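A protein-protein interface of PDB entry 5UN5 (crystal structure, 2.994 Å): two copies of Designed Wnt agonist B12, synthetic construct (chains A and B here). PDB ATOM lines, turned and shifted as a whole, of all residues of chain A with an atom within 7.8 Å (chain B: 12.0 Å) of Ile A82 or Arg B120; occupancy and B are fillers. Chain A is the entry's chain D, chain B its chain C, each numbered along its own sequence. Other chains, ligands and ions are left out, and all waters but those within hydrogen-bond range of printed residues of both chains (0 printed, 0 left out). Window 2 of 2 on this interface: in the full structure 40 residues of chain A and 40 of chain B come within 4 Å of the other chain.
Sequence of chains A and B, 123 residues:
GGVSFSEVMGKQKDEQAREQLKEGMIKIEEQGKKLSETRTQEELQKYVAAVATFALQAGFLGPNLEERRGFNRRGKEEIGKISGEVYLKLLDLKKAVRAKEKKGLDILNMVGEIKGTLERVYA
The side-chain hydroxyl (OG1) of Thr B117 sits at hydrogen-bond distance from the backbone carbonyl oxygen (O) of Glu B113, 3.0 Å away.
No position is printed for both chains.
Of the 9 pairs that touch across the chains among the printed residues, none has its exchanged pair printed and touching as well.
Phe A54 touches Leu B21 (CE1 to O, 3.5 Å).
Met B25 touches Phe A54.
Phe A54 touches Ile B28.
Phe A54 touches Leu B118.
CG2 of Val B121 touches CE2 of Phe A54 (3.9 Å).
Val B121 touches Ala A58 (CG1 to CB, 3.9 Å).
Ile A82 touches Arg B120 (CD1 to CB, 3.9 Å).
Glu A85 touches Thr B117.
Val A86 touches Thr B117.
Of the printed residues of chain B, Phe A54 touches Leu B21 (3.5 Å), Met B25 (3.9 Å), Ile B28 (3.7 Å), Leu B118 (3.9 Å) and Val B121 (3.9 Å).
Of the printed residues of chain B, Ala A58 touches Val B121 (3.9 Å).
No residue of chain B comes within 4 Å of Gly A80.
No residue of chain B comes within 4 Å of Lys A81.
Of the printed residues of chain B, Ile A82 touches Arg B120 (3.9 Å).
No residue of chain B comes within 4 Å of Ser A83.
Of the printed residues of chain B, Glu A85 touches Thr B117.
Printed residues of chain A within 4 Å of Met B25: Phe A54 (3.9 Å).
Arg B120 touches one residue of chain A.
Printed residues of chain A within 4 Å of Val B121: Phe A54 and Ala A58.
The nearest residue of chain A that does not touch Arg B120 is Glu A85 (7.1 Å).
The nearest printed residue of chain A that does not touch Val B121 is Phe A60 (4.5 Å).
Along chain B the printed residues that touch a printed residue of chain A span positions 21 to 121.
Among the printed residues, 9 pairs touch across the chains.
Among the printed residues, no Asp or Glu carboxylate lies within 4 Å of a Lys or Arg side-chain nitrogen of the other chain.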
ATOM      1  N   PHE A  54      22.294   5.429   8.353  1.00  0.00           N
ATOM      2  CA  PHE A  54      21.348   5.555   7.250  1.00  0.00           C
ATOM      3  C   PHE A  54      22.070   5.867   5.945  1.00  0.00           C
ATOM      4  O   PHE A  54      21.687   5.368   4.879  1.00  0.00           O
ATOM      5  CB  PHE A  54      20.316   6.637   7.574  1.00  0.00           C
ATOM      6  CG  PHE A  54      19.291   6.848   6.495  1.00  0.00           C
ATOM      7  CD1 PHE A  54      18.135   6.086   6.462  1.00  0.00           C
ATOM      8  CD2 PHE A  54      19.474   7.819   5.522  1.00  0.00           C
ATOM      9  CE1 PHE A  54      17.188   6.280   5.477  1.00  0.00           C
ATOM     10  CE2 PHE A  54      18.531   8.016   4.533  1.00  0.00           C
ATOM     11  CZ  PHE A  54      17.386   7.246   4.511  1.00  0.00           C
ATOM     12  N   ALA A  58      21.777   3.570   2.535  1.00  0.00           N
ATOM     13  CA  ALA A  58      21.343   4.153   1.272  1.00  0.00           C
ATOM     14  C   ALA A  58      22.420   4.121   0.196  1.00  0.00           C
ATOM     15  O   ALA A  58      22.147   4.521  -0.941  1.00  0.00           O
ATOM     16  CB  ALA A  58      20.875   5.593   1.491  1.00  0.00           C
ATOM     17  N   PHE A  60      25.624   5.728   0.114  1.00  0.00           N
ATOM     18  CA  PHE A  60      26.250   7.012  -0.182  1.00  0.00           C
ATOM     19  C   PHE A  60      27.689   6.861  -0.661  1.00  0.00           C
ATOM     20  O   PHE A  60      28.255   7.819  -1.199  1.00  0.00           O
ATOM     21  CB  PHE A  60      26.231   7.920   1.050  1.00  0.00           C
ATOM     22  CG  PHE A  60      24.914   8.602   1.292  1.00  0.00           C
ATOM     23  CD1 PHE A  60      23.735   8.081   0.784  1.00  0.00           C
ATOM     24  CD2 PHE A  60      24.859   9.769   2.037  1.00  0.00           C
ATOM     25  CE1 PHE A  60      22.530   8.710   1.018  1.00  0.00           C
ATOM     26  CE2 PHE A  60      23.655  10.402   2.271  1.00  0.00           C
ATOM     27  CZ  PHE A  60      22.489   9.870   1.762  1.00  0.00           C
ATOM     28  N   GLU A  78      24.493  10.491  -9.092  1.00  0.00           N
ATOM     29  CA  GLU A  78      23.465  11.476  -8.784  1.00  0.00           C
ATOM     30  C   GLU A  78      23.250  11.568  -7.279  1.00  0.00           C
ATOM     31  O   GLU A  78      22.926  12.631  -6.750  1.00  0.00           O
ATOM     32  CB  GLU A  78      22.153  11.118  -9.483  1.00  0.00           C
ATOM     33  N   ILE A  79      23.432  10.435  -6.595  1.00  0.00           N
ATOM     34  CA  ILE A  79      23.265  10.407  -5.146  1.00  0.00           C
ATOM     35  C   ILE A  79      24.389  11.182  -4.469  1.00  0.00           C
ATOM     36  O   ILE A  79      24.224  11.681  -3.349  1.00  0.00           O
ATOM     37  CB  ILE A  79      23.174   8.954  -4.643  1.00  0.00           C
ATOM     38  CG1 ILE A  79      22.738   8.925  -3.174  1.00  0.00           C
ATOM     39  CG2 ILE A  79      24.496   8.227  -4.845  1.00  0.00           C
ATOM     40  CD1 ILE A  79      22.393   7.547  -2.664  1.00  0.00           C
ATOM     41  N   GLY A  80      25.543  11.295  -5.135  1.00  0.00           N
ATOM     42  CA  GLY A  80      26.663  12.039  -4.575  1.00  0.00           C
ATOM     43  C   GLY A  80      26.300  13.456  -4.180  1.00  0.00           C
ATOM     44  O   GLY A  80      26.796  13.977  -3.179  1.00  0.00           O
ATOM     45  N   LYS A  81      25.446  14.109  -4.973  1.00  0.00           N
ATOM     46  CA  LYS A  81      24.988  15.446  -4.608  1.00  0.00           C
ATOM     47  C   LYS A  81      24.179  15.412  -3.317  1.00  0.00           C
ATOM     48  O   LYS A  81      24.312  16.304  -2.471  1.00  0.00           O
ATOM     49  CB  LYS A  81      24.163  16.048  -5.746  1.00  0.00           C
ATOM     50  N   ILE A  82      23.339  14.389  -3.148  1.00  0.00           N
ATOM     51  CA  ILE A  82      22.583  14.247  -1.905  1.00  0.00           C
ATOM     52  C   ILE A  82      23.531  14.005  -0.737  1.00  0.00           C
ATOM     53  O   ILE A  82      23.372  14.585   0.344  1.00  0.00           O
ATOM     54  CB  ILE A  82      21.543  13.120  -2.033  1.00  0.00           C
ATOM     55  CG1 ILE A  82      20.559  13.424  -3.163  1.00  0.00           C
ATOM     56  CG2 ILE A  82      20.800  12.925  -0.718  1.00  0.00           C
ATOM     57  CD1 ILE A  82      19.444  12.408  -3.290  1.00  0.00           C
ATOM     58  N   SER A  83      24.529  13.139  -0.935  1.00  0.00           N
ATOM     59  CA  SER A  83      25.496  12.858   0.121  1.00  0.00           C
ATOM     60  C   SER A  83      26.262  14.114   0.519  1.00  0.00           C
ATOM     61  O   SER A  83      26.550  14.326   1.703  1.00  0.00           O
ATOM     62  CB  SER A  83      26.461  11.763  -0.335  1.00  0.00           C
ATOM     63  OG  SER A  83      27.329  11.375   0.714  1.00  0.00           O
ATOM     64  N   GLY A  84      26.602  14.956  -0.457  1.00  0.00           N
ATOM     65  CA  GLY A  84      27.313  16.185  -0.144  1.00  0.00           C
ATOM     66  C   GLY A  84      26.473  17.162   0.655  1.00  0.00           C
ATOM     67  O   GLY A  84      26.978  17.831   1.561  1.00  0.00           O
ATOM     68  N   GLU A  85      25.181  17.258   0.333  1.00  0.00           N
ATOM     69  CA  GLU A  85      24.306  18.174   1.059  1.00  0.00           C
ATOM     70  C   GLU A  85      24.090  17.726   2.499  1.00  0.00           C
ATOM     71  O   GLU A  85      23.942  18.569   3.392  1.00  0.00           O
ATOM     72  CB  GLU A  85      22.965  18.308   0.338  1.00  0.00           C
ATOM     73  CG  GLU A  85      23.067  18.929  -1.046  1.00  0.00           C
ATOM     74  CD  GLU A  85      21.725  19.009  -1.748  1.00  0.00           C
ATOM     75  OE1 GLU A  85      20.721  18.542  -1.169  1.00  0.00           O
ATOM     76  OE2 GLU A  85      21.674  19.539  -2.879  1.00  0.00           O
ATOM     77  N   VAL A  86      24.066  16.415   2.745  1.00  0.00           N
ATOM     78  CA  VAL A  86      23.858  15.915   4.100  1.00  0.00           C
ATOM     79  C   VAL A  86      25.055  16.253   4.982  1.00  0.00           C
ATOM     80  O   VAL A  86      24.898  16.718   6.117  1.00  0.00           O
ATOM     81  CB  VAL A  86      23.583  14.400   4.077  1.00  0.00           C
ATOM     82  CG1 VAL A  86      23.525  13.848   5.491  1.00  0.00           C
ATOM     83  CG2 VAL A  86      22.286  14.107   3.338  1.00  0.00           C
ATOM     84  N   TYR A  87      26.267  16.025   4.472  1.00  0.00           N
ATOM     85  CA  TYR A  87      27.463  16.270   5.273  1.00  0.00           C
ATOM     86  C   TYR A  87      27.642  17.752   5.575  1.00  0.00           C
ATOM     87  O   TYR A  87      28.067  18.118   6.677  1.00  0.00           O
ATOM     88  CB  TYR A  87      28.697  15.714   4.562  1.00  0.00           C
ATOM     89  CG  TYR A  87      29.976  15.903   5.343  1.00  0.00           C
ATOM     90  CD1 TYR A  87      30.150  15.303   6.583  1.00  0.00           C
ATOM     91  CD2 TYR A  87      31.010  16.683   4.842  1.00  0.00           C
ATOM     92  CE1 TYR A  87      31.318  15.473   7.301  1.00  0.00           C
ATOM     93  CE2 TYR A  87      32.182  16.859   5.551  1.00  0.00           C
ATOM     94  CZ  TYR A  87      32.330  16.252   6.780  1.00  0.00           C
ATOM     95  OH  TYR A  87      33.496  16.425   7.490  1.00  0.00           O
ATOM     96  N   LEU A  88      27.326  18.621   4.611  1.00  0.00           N
ATOM     97  CA  LEU A  88      27.455  20.055   4.848  1.00  0.00           C
ATOM     98  C   LEU A  88      26.472  20.531   5.911  1.00  0.00           C
ATOM     99  O   LEU A  88      26.810  21.390   6.736  1.00  0.00           O
ATOM    100  CB  LEU A  88      27.257  20.824   3.543  1.00  0.00           C
ATOM    101  CG  LEU A  88      28.350  20.626   2.491  1.00  0.00           C
ATOM    102  CD1 LEU A  88      28.056  21.443   1.241  1.00  0.00           C
ATOM    103  CD2 LEU A  88      29.722  20.971   3.055  1.00  0.00           C
ATOM    104  N   ARG B  18      13.617  -1.849   2.120  1.00  0.00           N
ATOM    105  CA  ARG B  18      13.017  -0.527   2.254  1.00  0.00           C
ATOM    106  C   ARG B  18      12.508  -0.288   3.669  1.00  0.00           C
ATOM    107  O   ARG B  18      12.560   0.843   4.166  1.00  0.00           O
ATOM    108  CB  ARG B  18      11.881  -0.358   1.244  1.00  0.00           C
ATOM    109  N   LEU B  21      15.411   0.795   5.931  1.00  0.00           N
ATOM    110  CA  LEU B  21      15.705   2.219   5.811  1.00  0.00           C
ATOM    111  C   LEU B  21      14.670   3.054   6.549  1.00  0.00           C
ATOM    112  O   LEU B  21      14.994   4.130   7.065  1.00  0.00           O
ATOM    113  CB  LEU B  21      15.771   2.629   4.338  1.00  0.00           C
ATOM    114  CG  LEU B  21      17.113   2.483   3.613  1.00  0.00           C
ATOM    115  CD1 LEU B  21      17.522   1.023   3.473  1.00  0.00           C
ATOM    116  CD2 LEU B  21      17.057   3.160   2.250  1.00  0.00           C
ATOM    117  N   LYS B  22      13.423   2.581   6.603  1.00  0.00           N
ATOM    118  CA  LYS B  22      12.410   3.260   7.403  1.00  0.00           C
ATOM    119  C   LYS B  22      12.751   3.175   8.884  1.00  0.00           C
ATOM    120  O   LYS B  22      12.570   4.148   9.626  1.00  0.00           O
ATOM    121  CB  LYS B  22      11.030   2.663   7.127  1.00  0.00           C
ATOM    122  N   MET B  25      15.265   5.561   9.566  1.00  0.00           N
ATOM    123  CA  MET B  25      14.713   6.912   9.609  1.00  0.00           C
ATOM    124  C   MET B  25      14.090   7.215  10.966  1.00  0.00           C
ATOM    125  O   MET B  25      14.261   8.318  11.499  1.00  0.00           O
ATOM    126  CB  MET B  25      13.687   7.094   8.492  1.00  0.00           C
ATOM    127  CG  MET B  25      13.089   8.486   8.430  1.00  0.00           C
ATOM    128  SD  MET B  25      14.336   9.737   8.073  1.00  0.00           S
ATOM    129  CE  MET B  25      14.711   9.362   6.362  1.00  0.00           C
ATOM    130  N   ILE B  28      16.690   8.048  13.398  1.00  0.00           N
ATOM    131  CA  ILE B  28      17.139   9.429  13.270  1.00  0.00           C
ATOM    132  C   ILE B  28      16.140  10.380  13.918  1.00  0.00           C
ATOM    133  O   ILE B  28      16.526  11.305  14.643  1.00  0.00           O
ATOM    134  CB  ILE B  28      17.377   9.768  11.788  1.00  0.00           C
ATOM    135  CG1 ILE B  28      18.542   8.939  11.246  1.00  0.00           C
ATOM    136  CG2 ILE B  28      17.641  11.253  11.612  1.00  0.00           C
ATOM    137  CD1 ILE B  28      18.824   9.165   9.785  1.00  0.00           C
ATOM    138  N   VAL B 111      17.853  20.146  12.155  1.00  0.00           N
ATOM    139  CA  VAL B 111      17.517  18.729  12.067  1.00  0.00           C
ATOM    140  C   VAL B 111      16.254  18.515  11.246  1.00  0.00           C
ATOM    141  O   VAL B 111      16.059  17.429  10.689  1.00  0.00           O
ATOM    142  CB  VAL B 111      17.368  18.099  13.466  1.00  0.00           C
ATOM    143  CG1 VAL B 111      18.642  18.289  14.277  1.00  0.00           C
ATOM    144  CG2 VAL B 111      16.168  18.674  14.198  1.00  0.00           C
ATOM    145  N   GLY B 112      15.390  19.528  11.150  1.00  0.00           N
ATOM    146  CA  GLY B 112      14.260  19.437  10.243  1.00  0.00           C
ATOM    147  C   GLY B 112      14.688  19.466   8.788  1.00  0.00           C
ATOM    148  O   GLY B 112      14.169  18.709   7.963  1.00  0.00           O
ATOM    149  N   GLU B 113      15.636  20.347   8.451  1.00  0.00           N
ATOM    150  CA  GLU B 113      16.147  20.395   7.085  1.00  0.00           C
ATOM    151  C   GLU B 113      16.906  19.126   6.723  1.00  0.00           C
ATOM    152  O   GLU B 113      16.879  18.699   5.563  1.00  0.00           O
ATOM    153  CB  GLU B 113      17.054  21.612   6.896  1.00  0.00           C
ATOM    154  CG  GLU B 113      16.345  22.951   6.984  1.00  0.00           C
ATOM    155  CD  GLU B 113      17.274  24.116   6.694  1.00  0.00           C
ATOM    156  OE1 GLU B 113      18.490  23.882   6.536  1.00  0.00           O
ATOM    157  OE2 GLU B 113      16.786  25.264   6.621  1.00  0.00           O
ATOM    158  N   ILE B 114      17.585  18.512   7.695  1.00  0.00           N
ATOM    159  CA  ILE B 114      18.294  17.266   7.430  1.00  0.00           C
ATOM    160  C   ILE B 114      17.308  16.147   7.128  1.00  0.00           C
ATOM    161  O   ILE B 114      17.528  15.335   6.221  1.00  0.00           O
ATOM    162  CB  ILE B 114      19.217  16.910   8.609  1.00  0.00           C
ATOM    163  CG1 ILE B 114      20.322  17.956   8.758  1.00  0.00           C
ATOM    164  CG2 ILE B 114      19.828  15.529   8.414  1.00  0.00           C
ATOM    165  CD1 ILE B 114      21.294  17.660   9.877  1.00  0.00           C
ATOM    166  N   LYS B 115      16.198  16.093   7.869  1.00  0.00           N
ATOM    167  CA  LYS B 115      15.180  15.085   7.592  1.00  0.00           C
ATOM    168  C   LYS B 115      14.607  15.256   6.191  1.00  0.00           C
ATOM    169  O   LYS B 115      14.356  14.268   5.491  1.00  0.00           O
ATOM    170  CB  LYS B 115      14.067  15.161   8.639  1.00  0.00           C
ATOM    171  N   GLY B 116      14.418  16.505   5.758  1.00  0.00           N
ATOM    172  CA  GLY B 116      13.937  16.746   4.408  1.00  0.00           C
ATOM    173  C   GLY B 116      14.909  16.273   3.346  1.00  0.00           C
ATOM    174  O   GLY B 116      14.508  15.672   2.346  1.00  0.00           O
ATOM    175  N   THR B 117      16.201  16.551   3.536  1.00  0.00           N
ATOM    176  CA  THR B 117      17.198  16.072   2.586  1.00  0.00           C
ATOM    177  C   THR B 117      17.264  14.551   2.574  1.00  0.00           C
ATOM    178  O   THR B 117      17.497  13.946   1.521  1.00  0.00           O
ATOM    179  CB  THR B 117      18.565  16.672   2.913  1.00  0.00           C
ATOM    180  OG1 THR B 117      18.440  18.093   3.038  1.00  0.00           O
ATOM    181  CG2 THR B 117      19.566  16.357   1.809  1.00  0.00           C
ATOM    182  N   LEU B 118      17.047  13.912   3.725  1.00  0.00           N
ATOM    183  CA  LEU B 118      17.037  12.457   3.770  1.00  0.00           C
ATOM    184  C   LEU B 118      15.787  11.883   3.118  1.00  0.00           C
ATOM    185  O   LEU B 118      15.775  10.702   2.760  1.00  0.00           O
ATOM    186  CB  LEU B 118      17.145  11.978   5.219  1.00  0.00           C
ATOM    187  CG  LEU B 118      18.462  12.283   5.941  1.00  0.00           C
ATOM    188  CD1 LEU B 118      18.417  11.769   7.369  1.00  0.00           C
ATOM    189  CD2 LEU B 118      19.666  11.702   5.205  1.00  0.00           C
ATOM    190  N   GLU B 119      14.741  12.698   2.950  1.00  0.00           N
ATOM    191  CA  GLU B 119      13.510  12.230   2.325  1.00  0.00           C
ATOM    192  C   GLU B 119      13.695  11.949   0.839  1.00  0.00           C
ATOM    193  O   GLU B 119      12.926  11.168   0.268  1.00  0.00           O
ATOM    194  CB  GLU B 119      12.386  13.256   2.507  1.00  0.00           C
ATOM    195  CG  GLU B 119      11.787  13.371   3.917  1.00  0.00           C
ATOM    196  CD  GLU B 119      11.369  12.047   4.544  1.00  0.00           C
ATOM    197  OE1 GLU B 119      11.107  11.067   3.813  1.00  0.00           O
ATOM    198  OE2 GLU B 119      11.296  11.996   5.791  1.00  0.00           O
ATOM    199  N   ARG B 120      14.685  12.577   0.197  1.00  0.00           N
ATOM    200  CA  ARG B 120      14.907  12.361  -1.230  1.00  0.00           C
ATOM    201  C   ARG B 120      15.285  10.917  -1.540  1.00  0.00           C
ATOM    202  O   ARG B 120      15.119  10.466  -2.680  1.00  0.00           O
ATOM    203  CB  ARG B 120      15.993  13.312  -1.739  1.00  0.00           C
ATOM    204  N   VAL B 121      15.786  10.179  -0.555  1.00  0.00           N
ATOM    205  CA  VAL B 121      16.149   8.781  -0.764  1.00  0.00           C
ATOM    206  C   VAL B 121      14.904   7.939  -1.027  1.00  0.00           C
ATOM    207  O   VAL B 121      14.161   7.603  -0.103  1.00  0.00           O
ATOM    208  CB  VAL B 121      16.935   8.220   0.434  1.00  0.00           C
ATOM    209  CG1 VAL B 121      17.492   6.839   0.105  1.00  0.00           C
ATOM    210  CG2 VAL B 121      18.048   9.172   0.830  1.00  0.00           C
